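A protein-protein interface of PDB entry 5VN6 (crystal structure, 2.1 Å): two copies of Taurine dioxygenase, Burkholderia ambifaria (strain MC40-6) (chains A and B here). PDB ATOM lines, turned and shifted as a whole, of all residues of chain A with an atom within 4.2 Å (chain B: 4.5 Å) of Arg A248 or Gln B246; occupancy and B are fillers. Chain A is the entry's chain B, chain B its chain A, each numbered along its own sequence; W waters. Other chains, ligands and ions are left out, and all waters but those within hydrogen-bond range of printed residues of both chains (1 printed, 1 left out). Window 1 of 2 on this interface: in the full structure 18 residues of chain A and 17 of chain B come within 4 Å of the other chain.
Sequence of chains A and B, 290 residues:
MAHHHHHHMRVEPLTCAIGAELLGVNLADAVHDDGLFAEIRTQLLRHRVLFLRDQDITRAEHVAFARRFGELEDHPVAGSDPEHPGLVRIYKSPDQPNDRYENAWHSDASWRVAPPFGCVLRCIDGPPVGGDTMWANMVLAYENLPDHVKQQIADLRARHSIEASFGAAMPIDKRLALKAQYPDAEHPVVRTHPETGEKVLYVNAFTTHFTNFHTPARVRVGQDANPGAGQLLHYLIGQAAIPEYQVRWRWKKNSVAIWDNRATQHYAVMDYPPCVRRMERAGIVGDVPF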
ATOM      1  N   ASP A 132      -2.990 -23.021 -18.512  1.00  0.00           N
ATOM      2  CA  ASP A 132      -1.698 -23.133 -17.848  1.00  0.00           C
ATOM      3  C   ASP A 132      -1.845 -22.863 -16.350  1.00  0.00           C
ATOM      4  O   ASP A 132      -2.771 -22.188 -15.906  1.00  0.00           O
ATOM      5  CB  ASP A 132      -0.701 -22.129 -18.426  1.00  0.00           C
ATOM      6  CG  ASP A 132      -0.260 -22.462 -19.854  1.00  0.00           C
ATOM      7  OD1 ASP A 132      -0.704 -23.463 -20.460  1.00  0.00           O
ATOM      8  OD2 ASP A 132       0.546 -21.683 -20.380  1.00  0.00           O
ATOM      9  N   THR A 133      -0.892 -23.375 -15.572  1.00  0.00           N
ATOM     10  CA  THR A 133      -0.784 -23.070 -14.152  1.00  0.00           C
ATOM     11  C   THR A 133       0.572 -22.429 -13.910  1.00  0.00           C
ATOM     12  O   THR A 133       1.556 -22.770 -14.577  1.00  0.00           O
ATOM     13  CB  THR A 133      -0.951 -24.334 -13.270  1.00  0.00           C
ATOM     14  OG1 THR A 133      -2.188 -24.965 -13.587  1.00  0.00           O
ATOM     15  CG2 THR A 133      -0.926 -23.994 -11.770  1.00  0.00           C
ATOM     16  N   MET A 134       0.596 -21.448 -13.015  1.00  0.00           N
ATOM     17  CA  MET A 134       1.804 -20.733 -12.635  1.00  0.00           C
ATOM     18  C   MET A 134       2.028 -20.871 -11.137  1.00  0.00           C
ATOM     19  O   MET A 134       1.075 -20.940 -10.367  1.00  0.00           O
ATOM     20  CB  MET A 134       1.709 -19.232 -12.995  1.00  0.00           C
ATOM     21  CG  MET A 134       1.301 -18.910 -14.422  1.00  0.00           C
ATOM     22  SD  MET A 134       1.189 -17.096 -14.635  1.00  0.00           S
ATOM     23  CE  MET A 134       2.883 -16.629 -14.313  1.00  0.00           C
ATOM     24  N   VAL A 247       7.021 -19.208 -12.423  1.00  0.00           N
ATOM     25  CA  VAL A 247       7.152 -20.184 -13.497  1.00  0.00           C
ATOM     26  C   VAL A 247       5.763 -20.497 -14.040  1.00  0.00           C
ATOM     27  O   VAL A 247       4.774 -20.473 -13.303  1.00  0.00           O
ATOM     28  CB  VAL A 247       7.864 -21.462 -13.020  1.00  0.00           C
ATOM     29  CG1 VAL A 247       7.061 -22.144 -11.897  1.00  0.00           C
ATOM     30  CG2 VAL A 247       8.115 -22.383 -14.188  1.00  0.00           C
ATOM     31  N   ARG A 248       5.689 -20.787 -15.341  1.00  0.00           N
ATOM     32  CA  ARG A 248       4.428 -21.074 -16.019  1.00  0.00           C
ATOM     33  C   ARG A 248       4.521 -22.415 -16.727  1.00  0.00           C
ATOM     34  O   ARG A 248       5.436 -22.635 -17.520  1.00  0.00           O
ATOM     35  CB  ARG A 248       4.074 -19.972 -17.025  1.00  0.00           C
ATOM     36  CG  ARG A 248       2.781 -20.218 -17.807  1.00  0.00           C
ATOM     37  CD  ARG A 248       2.106 -18.907 -18.169  1.00  0.00           C
ATOM     38  NE  ARG A 248       0.899 -19.149 -18.957  1.00  0.00           N
ATOM     39  CZ  ARG A 248      -0.031 -18.233 -19.205  1.00  0.00           C
ATOM     40  NH1 ARG A 248       0.112 -16.992 -18.729  1.00  0.00           N
ATOM     41  NH2 ARG A 248      -1.105 -18.556 -19.923  1.00  0.00           N
ATOM     42  N   TRP A 249       3.564 -23.298 -16.460  1.00  0.00           N
ATOM     43  CA  TRP A 249       3.603 -24.682 -16.924  1.00  0.00           C
ATOM     44  C   TRP A 249       2.426 -24.946 -17.852  1.00  0.00           C
ATOM     45  O   TRP A 249       1.290 -24.559 -17.558  1.00  0.00           O
ATOM     46  CB  TRP A 249       3.593 -25.638 -15.717  1.00  0.00           C
ATOM     47  CG  TRP A 249       3.494 -27.133 -15.997  1.00  0.00           C
ATOM     48  CD1 TRP A 249       2.414 -27.942 -15.745  1.00  0.00           C
ATOM     49  CD2 TRP A 249       4.524 -27.996 -16.520  1.00  0.00           C
ATOM     50  NE1 TRP A 249       2.699 -29.241 -16.098  1.00  0.00           N
ATOM     51  CE2 TRP A 249       3.982 -29.299 -16.586  1.00  0.00           C
ATOM     52  CE3 TRP A 249       5.837 -27.788 -16.964  1.00  0.00           C
ATOM     53  CZ2 TRP A 249       4.720 -30.393 -17.052  1.00  0.00           C
ATOM     54  CZ3 TRP A 249       6.563 -28.876 -17.439  1.00  0.00           C
ATOM     55  CH2 TRP A 249       6.006 -30.160 -17.470  1.00  0.00           C
ATOM     56  N   VAL A 269      -4.449 -20.296 -14.638  1.00  0.00           N
ATOM     57  CA  VAL A 269      -4.815 -19.315 -15.646  1.00  0.00           C
ATOM     58  C   VAL A 269      -6.136 -19.705 -16.283  1.00  0.00           C
ATOM     59  O   VAL A 269      -6.319 -20.842 -16.733  1.00  0.00           O
ATOM     60  CB  VAL A 269      -3.708 -19.181 -16.696  1.00  0.00           C
ATOM     61  CG1 VAL A 269      -4.055 -18.063 -17.668  1.00  0.00           C
ATOM     62  CG2 VAL A 269      -2.383 -18.902 -15.999  1.00  0.00           C
ATOM     63  N   THR B  15      -1.001 -20.175 -25.841  1.00  0.00           N
ATOM     64  CA  THR B  15      -2.081 -19.875 -24.903  1.00  0.00           C
ATOM     65  C   THR B  15      -3.293 -19.478 -25.738  1.00  0.00           C
ATOM     66  O   THR B  15      -3.179 -19.258 -26.947  1.00  0.00           O
ATOM     67  CB  THR B  15      -1.728 -18.715 -23.956  1.00  0.00           C
ATOM     68  OG1 THR B  15      -1.788 -17.486 -24.697  1.00  0.00           O
ATOM     69  CG2 THR B  15      -0.306 -18.866 -23.390  1.00  0.00           C
ATOM     70  N   ILE B  18      -2.652 -15.221 -26.560  1.00  0.00           N
ATOM     71  CA  ILE B  18      -1.518 -14.553 -27.180  1.00  0.00           C
ATOM     72  C   ILE B  18      -0.400 -15.549 -27.442  1.00  0.00           C
ATOM     73  O   ILE B  18      -0.101 -16.410 -26.601  1.00  0.00           O
ATOM     74  CB  ILE B  18      -1.013 -13.377 -26.312  1.00  0.00           C
ATOM     75  CG1 ILE B  18       0.200 -12.707 -26.977  1.00  0.00           C
ATOM     76  CG2 ILE B  18      -0.655 -13.830 -24.881  1.00  0.00           C
ATOM     77  CD1 ILE B  18       0.552 -11.334 -26.410  1.00  0.00           C
ATOM     78  N   TRP B 105       6.757  -4.126 -17.400  1.00  0.00           N
ATOM     79  CA  TRP B 105       5.743  -4.208 -18.449  1.00  0.00           C
ATOM     80  C   TRP B 105       5.779  -2.929 -19.295  1.00  0.00           C
ATOM     81  O   TRP B 105       5.387  -1.856 -18.835  1.00  0.00           O
ATOM     82  CB  TRP B 105       4.370  -4.460 -17.833  1.00  0.00           C
ATOM     83  CG  TRP B 105       4.227  -5.908 -17.454  1.00  0.00           C
ATOM     84  CD1 TRP B 105       4.166  -6.433 -16.193  1.00  0.00           C
ATOM     85  CD2 TRP B 105       4.196  -7.022 -18.358  1.00  0.00           C
ATOM     86  NE1 TRP B 105       4.069  -7.809 -16.258  1.00  0.00           N
ATOM     87  CE2 TRP B 105       4.085  -8.192 -17.575  1.00  0.00           C
ATOM     88  CE3 TRP B 105       4.238  -7.139 -19.756  1.00  0.00           C
ATOM     89  CZ2 TRP B 105       4.019  -9.464 -18.140  1.00  0.00           C
ATOM     90  CZ3 TRP B 105       4.171  -8.404 -20.320  1.00  0.00           C
ATOM     91  CH2 TRP B 105       4.054  -9.557 -19.505  1.00  0.00           C
ATOM     92  N   MET B 134       8.388 -12.306 -21.605  1.00  0.00           N
ATOM     93  CA  MET B 134       6.938 -12.422 -21.574  1.00  0.00           C
ATOM     94  C   MET B 134       6.321 -11.320 -22.402  1.00  0.00           C
ATOM     95  O   MET B 134       6.893 -10.236 -22.527  1.00  0.00           O
ATOM     96  CB  MET B 134       6.387 -12.335 -20.143  1.00  0.00           C
ATOM     97  CG  MET B 134       7.063 -13.299 -19.180  1.00  0.00           C
ATOM     98  SD  MET B 134       6.395 -13.116 -17.522  1.00  0.00           S
ATOM     99  CE  MET B 134       4.692 -13.577 -17.815  1.00  0.00           C
ATOM    100  N   TRP B 135       5.151 -11.611 -22.976  1.00  0.00           N
ATOM    101  CA  TRP B 135       4.335 -10.625 -23.664  1.00  0.00           C
ATOM    102  C   TRP B 135       2.927 -10.643 -23.089  1.00  0.00           C
ATOM    103  O   TRP B 135       2.455 -11.674 -22.605  1.00  0.00           O
ATOM    104  CB  TRP B 135       4.257 -10.879 -25.202  1.00  0.00           C
ATOM    105  CG  TRP B 135       5.491 -10.559 -25.967  1.00  0.00           C
ATOM    106  CD1 TRP B 135       5.708  -9.459 -26.733  1.00  0.00           C
ATOM    107  CD2 TRP B 135       6.680 -11.366 -26.073  1.00  0.00           C
ATOM    108  NE1 TRP B 135       6.956  -9.519 -27.305  1.00  0.00           N
ATOM    109  CE2 TRP B 135       7.574 -10.677 -26.913  1.00  0.00           C
ATOM    110  CE3 TRP B 135       7.072 -12.596 -25.529  1.00  0.00           C
ATOM    111  CZ2 TRP B 135       8.844 -11.175 -27.231  1.00  0.00           C
ATOM    112  CZ3 TRP B 135       8.327 -13.088 -25.834  1.00  0.00           C
ATOM    113  CH2 TRP B 135       9.199 -12.381 -26.680  1.00  0.00           C
ATOM    114  N   ALA B 136       2.240  -9.497 -23.183  1.00  0.00           N
ATOM    115  CA  ALA B 136       0.864  -9.363 -22.737  1.00  0.00           C
ATOM    116  C   ALA B 136       0.028  -8.762 -23.867  1.00  0.00           C
ATOM    117  O   ALA B 136       0.502  -7.900 -24.615  1.00  0.00           O
ATOM    118  CB  ALA B 136       0.763  -8.488 -21.477  1.00  0.00           C
ATOM    119  N   ALA B 240      -1.528  -5.284 -17.447  1.00  0.00           N
ATOM    120  CA  ALA B 240      -0.543  -6.130 -18.110  1.00  0.00           C
ATOM    121  C   ALA B 240      -0.032  -7.227 -17.195  1.00  0.00           C
ATOM    122  O   ALA B 240       0.579  -8.180 -17.680  1.00  0.00           O
ATOM    123  CB  ALA B 240       0.658  -5.319 -18.612  1.00  0.00           C
ATOM    124  N   ALA B 241      -0.232  -7.113 -15.885  1.00  0.00           N
ATOM    125  CA  ALA B 241       0.251  -8.137 -14.972  1.00  0.00           C
ATOM    126  C   ALA B 241      -0.730  -9.310 -14.806  1.00  0.00           C
ATOM    127  O   ALA B 241      -0.478 -10.210 -13.991  1.00  0.00           O
ATOM    128  CB  ALA B 241       0.577  -7.506 -13.616  1.00  0.00           C
ATOM    129  N   ILE B 242      -1.815  -9.346 -15.571  1.00  0.00           N
ATOM    130  CA  ILE B 242      -2.845 -10.371 -15.422  1.00  0.00           C
ATOM    131  C   ILE B 242      -2.426 -11.599 -16.231  1.00  0.00           C
ATOM    132  O   ILE B 242      -2.319 -11.506 -17.464  1.00  0.00           O
ATOM    133  CB  ILE B 242      -4.225  -9.854 -15.856  1.00  0.00           C
ATOM    134  CG1 ILE B 242      -4.724  -8.815 -14.846  1.00  0.00           C
ATOM    135  CG2 ILE B 242      -5.228 -11.021 -16.012  1.00  0.00           C
ATOM    136  CD1 ILE B 242      -5.942  -7.984 -15.316  1.00  0.00           C
ATOM    137  N   PRO B 243      -2.192 -12.748 -15.593  1.00  0.00           N
ATOM    138  CA  PRO B 243      -1.666 -13.899 -16.341  1.00  0.00           C
ATOM    139  C   PRO B 243      -2.535 -14.336 -17.507  1.00  0.00           C
ATOM    140  O   PRO B 243      -1.999 -14.878 -18.486  1.00  0.00           O
ATOM    141  CB  PRO B 243      -1.562 -14.991 -15.267  1.00  0.00           C
ATOM    142  CG  PRO B 243      -1.356 -14.206 -13.987  1.00  0.00           C
ATOM    143  CD  PRO B 243      -2.248 -13.002 -14.145  1.00  0.00           C
ATOM    144  N   GLU B 244      -3.853 -14.099 -17.441  1.00  0.00           N
ATOM    145  CA  GLU B 244      -4.748 -14.452 -18.546  1.00  0.00           C
ATOM    146  C   GLU B 244      -4.335 -13.813 -19.867  1.00  0.00           C
ATOM    147  O   GLU B 244      -4.669 -14.334 -20.933  1.00  0.00           O
ATOM    148  CB  GLU B 244      -6.184 -14.035 -18.220  1.00  0.00           C
ATOM    149  CG  GLU B 244      -6.977 -15.102 -17.463  1.00  0.00           C
ATOM    150  CD  GLU B 244      -6.630 -15.155 -15.984  1.00  0.00           C
ATOM    151  OE1 GLU B 244      -5.863 -14.269 -15.513  1.00  0.00           O
ATOM    152  OE2 GLU B 244      -7.123 -16.078 -15.294  1.00  0.00           O
ATOM    153  N   TYR B 245      -3.633 -12.688 -19.828  1.00  0.00           N
ATOM    154  CA  TYR B 245      -3.274 -11.959 -21.043  1.00  0.00           C
ATOM    155  C   TYR B 245      -1.862 -12.260 -21.510  1.00  0.00           C
ATOM    156  O   TYR B 245      -1.392 -11.637 -22.472  1.00  0.00           O
ATOM    157  CB  TYR B 245      -3.395 -10.444 -20.810  1.00  0.00           C
ATOM    158  CG  TYR B 245      -4.720  -9.993 -20.256  1.00  0.00           C
ATOM    159  CD1 TYR B 245      -5.897 -10.723 -20.501  1.00  0.00           C
ATOM    160  CD2 TYR B 245      -4.804  -8.820 -19.490  1.00  0.00           C
ATOM    161  CE1 TYR B 245      -7.132 -10.298 -19.978  1.00  0.00           C
ATOM    162  CE2 TYR B 245      -6.013  -8.390 -18.982  1.00  0.00           C
ATOM    163  CZ  TYR B 245      -7.177  -9.128 -19.234  1.00  0.00           C
ATOM    164  OH  TYR B 245      -8.374  -8.683 -18.720  1.00  0.00           O
ATOM    165  N   GLN B 246      -1.172 -13.189 -20.850  1.00  0.00           N
ATOM    166  CA  GLN B 246       0.273 -13.296 -20.943  1.00  0.00           C
ATOM    167  C   GLN B 246       0.700 -14.582 -21.640  1.00  0.00           C
ATOM    168  O   GLN B 246       0.001 -15.600 -21.630  1.00  0.00           O
ATOM    169  CB  GLN B 246       0.927 -13.245 -19.547  1.00  0.00           C
ATOM    170  CG  GLN B 246       0.822 -11.888 -18.862  1.00  0.00           C
ATOM    171  CD  GLN B 246       1.347 -11.949 -17.434  1.00  0.00           C
ATOM    172  OE1 GLN B 246       1.719 -13.009 -16.959  1.00  0.00           O
ATOM    173  NE2 GLN B 246       1.318 -10.829 -16.731  1.00  0.00           N
ATOM    174  N   VAL B 247       1.902 -14.525 -22.211  1.00  0.00           N
ATOM    175  CA  VAL B 247       2.624 -15.713 -22.638  1.00  0.00           C
ATOM    176  C   VAL B 247       4.062 -15.549 -22.173  1.00  0.00           C
ATOM    177  O   VAL B 247       4.572 -14.429 -22.077  1.00  0.00           O
ATOM    178  CB  VAL B 247       2.538 -15.946 -24.170  1.00  0.00           C
ATOM    179  CG1 VAL B 247       3.144 -14.759 -24.995  1.00  0.00           C
ATOM    180  CG2 VAL B 247       3.201 -17.248 -24.550  1.00  0.00           C
HETATM  181  O   HOH W   1       2.211 -15.625 -17.327  1.00  0.00           O
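O of Pro B243 is in hydrogen-bond range of NH1 of Arg A248 (3.0 Å). The backbone carbonyl oxygen of Gln B246 is in hydrogen-bond range of the guanidinium group of Arg A248 (3.2 Å).
The side-chain hydroxyl of Thr B15 lies within hydrogen-bond range of the backbone carbonyl oxygen of Ile B18 (2.8 Å). The backbone carbonyl oxygen (O) of Ala B240 sits at hydrogen-bond distance from the side-chain amide nitrogen (NE2) of Gln B246, at 2.9 Å. O of Ala B241 lies close to NE2 of Gln B246, 3.3 Å away. OD2 of Asp A132 lies within salt-bridge range of NE of Arg A248, at 2.9 Å. The backbone carbonyl oxygen (O) of Asp A132 sits at hydrogen-bond distance from the backbone NH (N) of Val A269, 2.8 Å away.
Among the printed residues, pairs that only touch across the chains: Met A134 with Pro B243, Arg A248 with Thr B15, Val A269 with Pro B243 and Val A269 with Glu B244.
Printed residues of chain A within 4 Å of Pro B243: Met A134 (3.5 Å), Arg A248 (3.0 Å) and Val A269 (3.9 Å). Of the printed residues of chain B, Met A134 touches Pro B243 (3.5 Å). Of the printed residues of chain B, Val A269 touches Pro B243 (3.9 Å) and Glu B244 (3.8 Å). Printed residues of chain A within 4 Å of Thr B15: Arg A248. Printed residues of chain A within 4 Å of Glu B244: Val A269 (3.8 Å). The nearest printed residue of chain B that does not touch Arg A248 is Val B247 (4.6 Å).
Printed residues of chain B that touch a printed residue of chain A: Thr B15, Pro B243, Glu B244 and Gln B246. Hydrophobic or aromatic side chains of chain B within 4 Å of the printed part of chain A: Pro B243. Along chain B the printed residues that touch a printed residue of chain A span positions 15 to 246. Of the 7 printed residues of chain A, 3 touch a printed residue of chain B.
2 positions are printed for both chains. Of the 6 pairs that touch across the chains among the printed residues, none has its exchanged pair printed and touching as well.
Water W1 lies within hydrogen-bond range of the side-chain amide oxygen (OE1) of Gln B246 (2.7 Å), the guanidinium group (NH1) of Arg A248 (2.9 Å) and the side-chain sulfur (SD) of Met A134 (3.2 Å).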
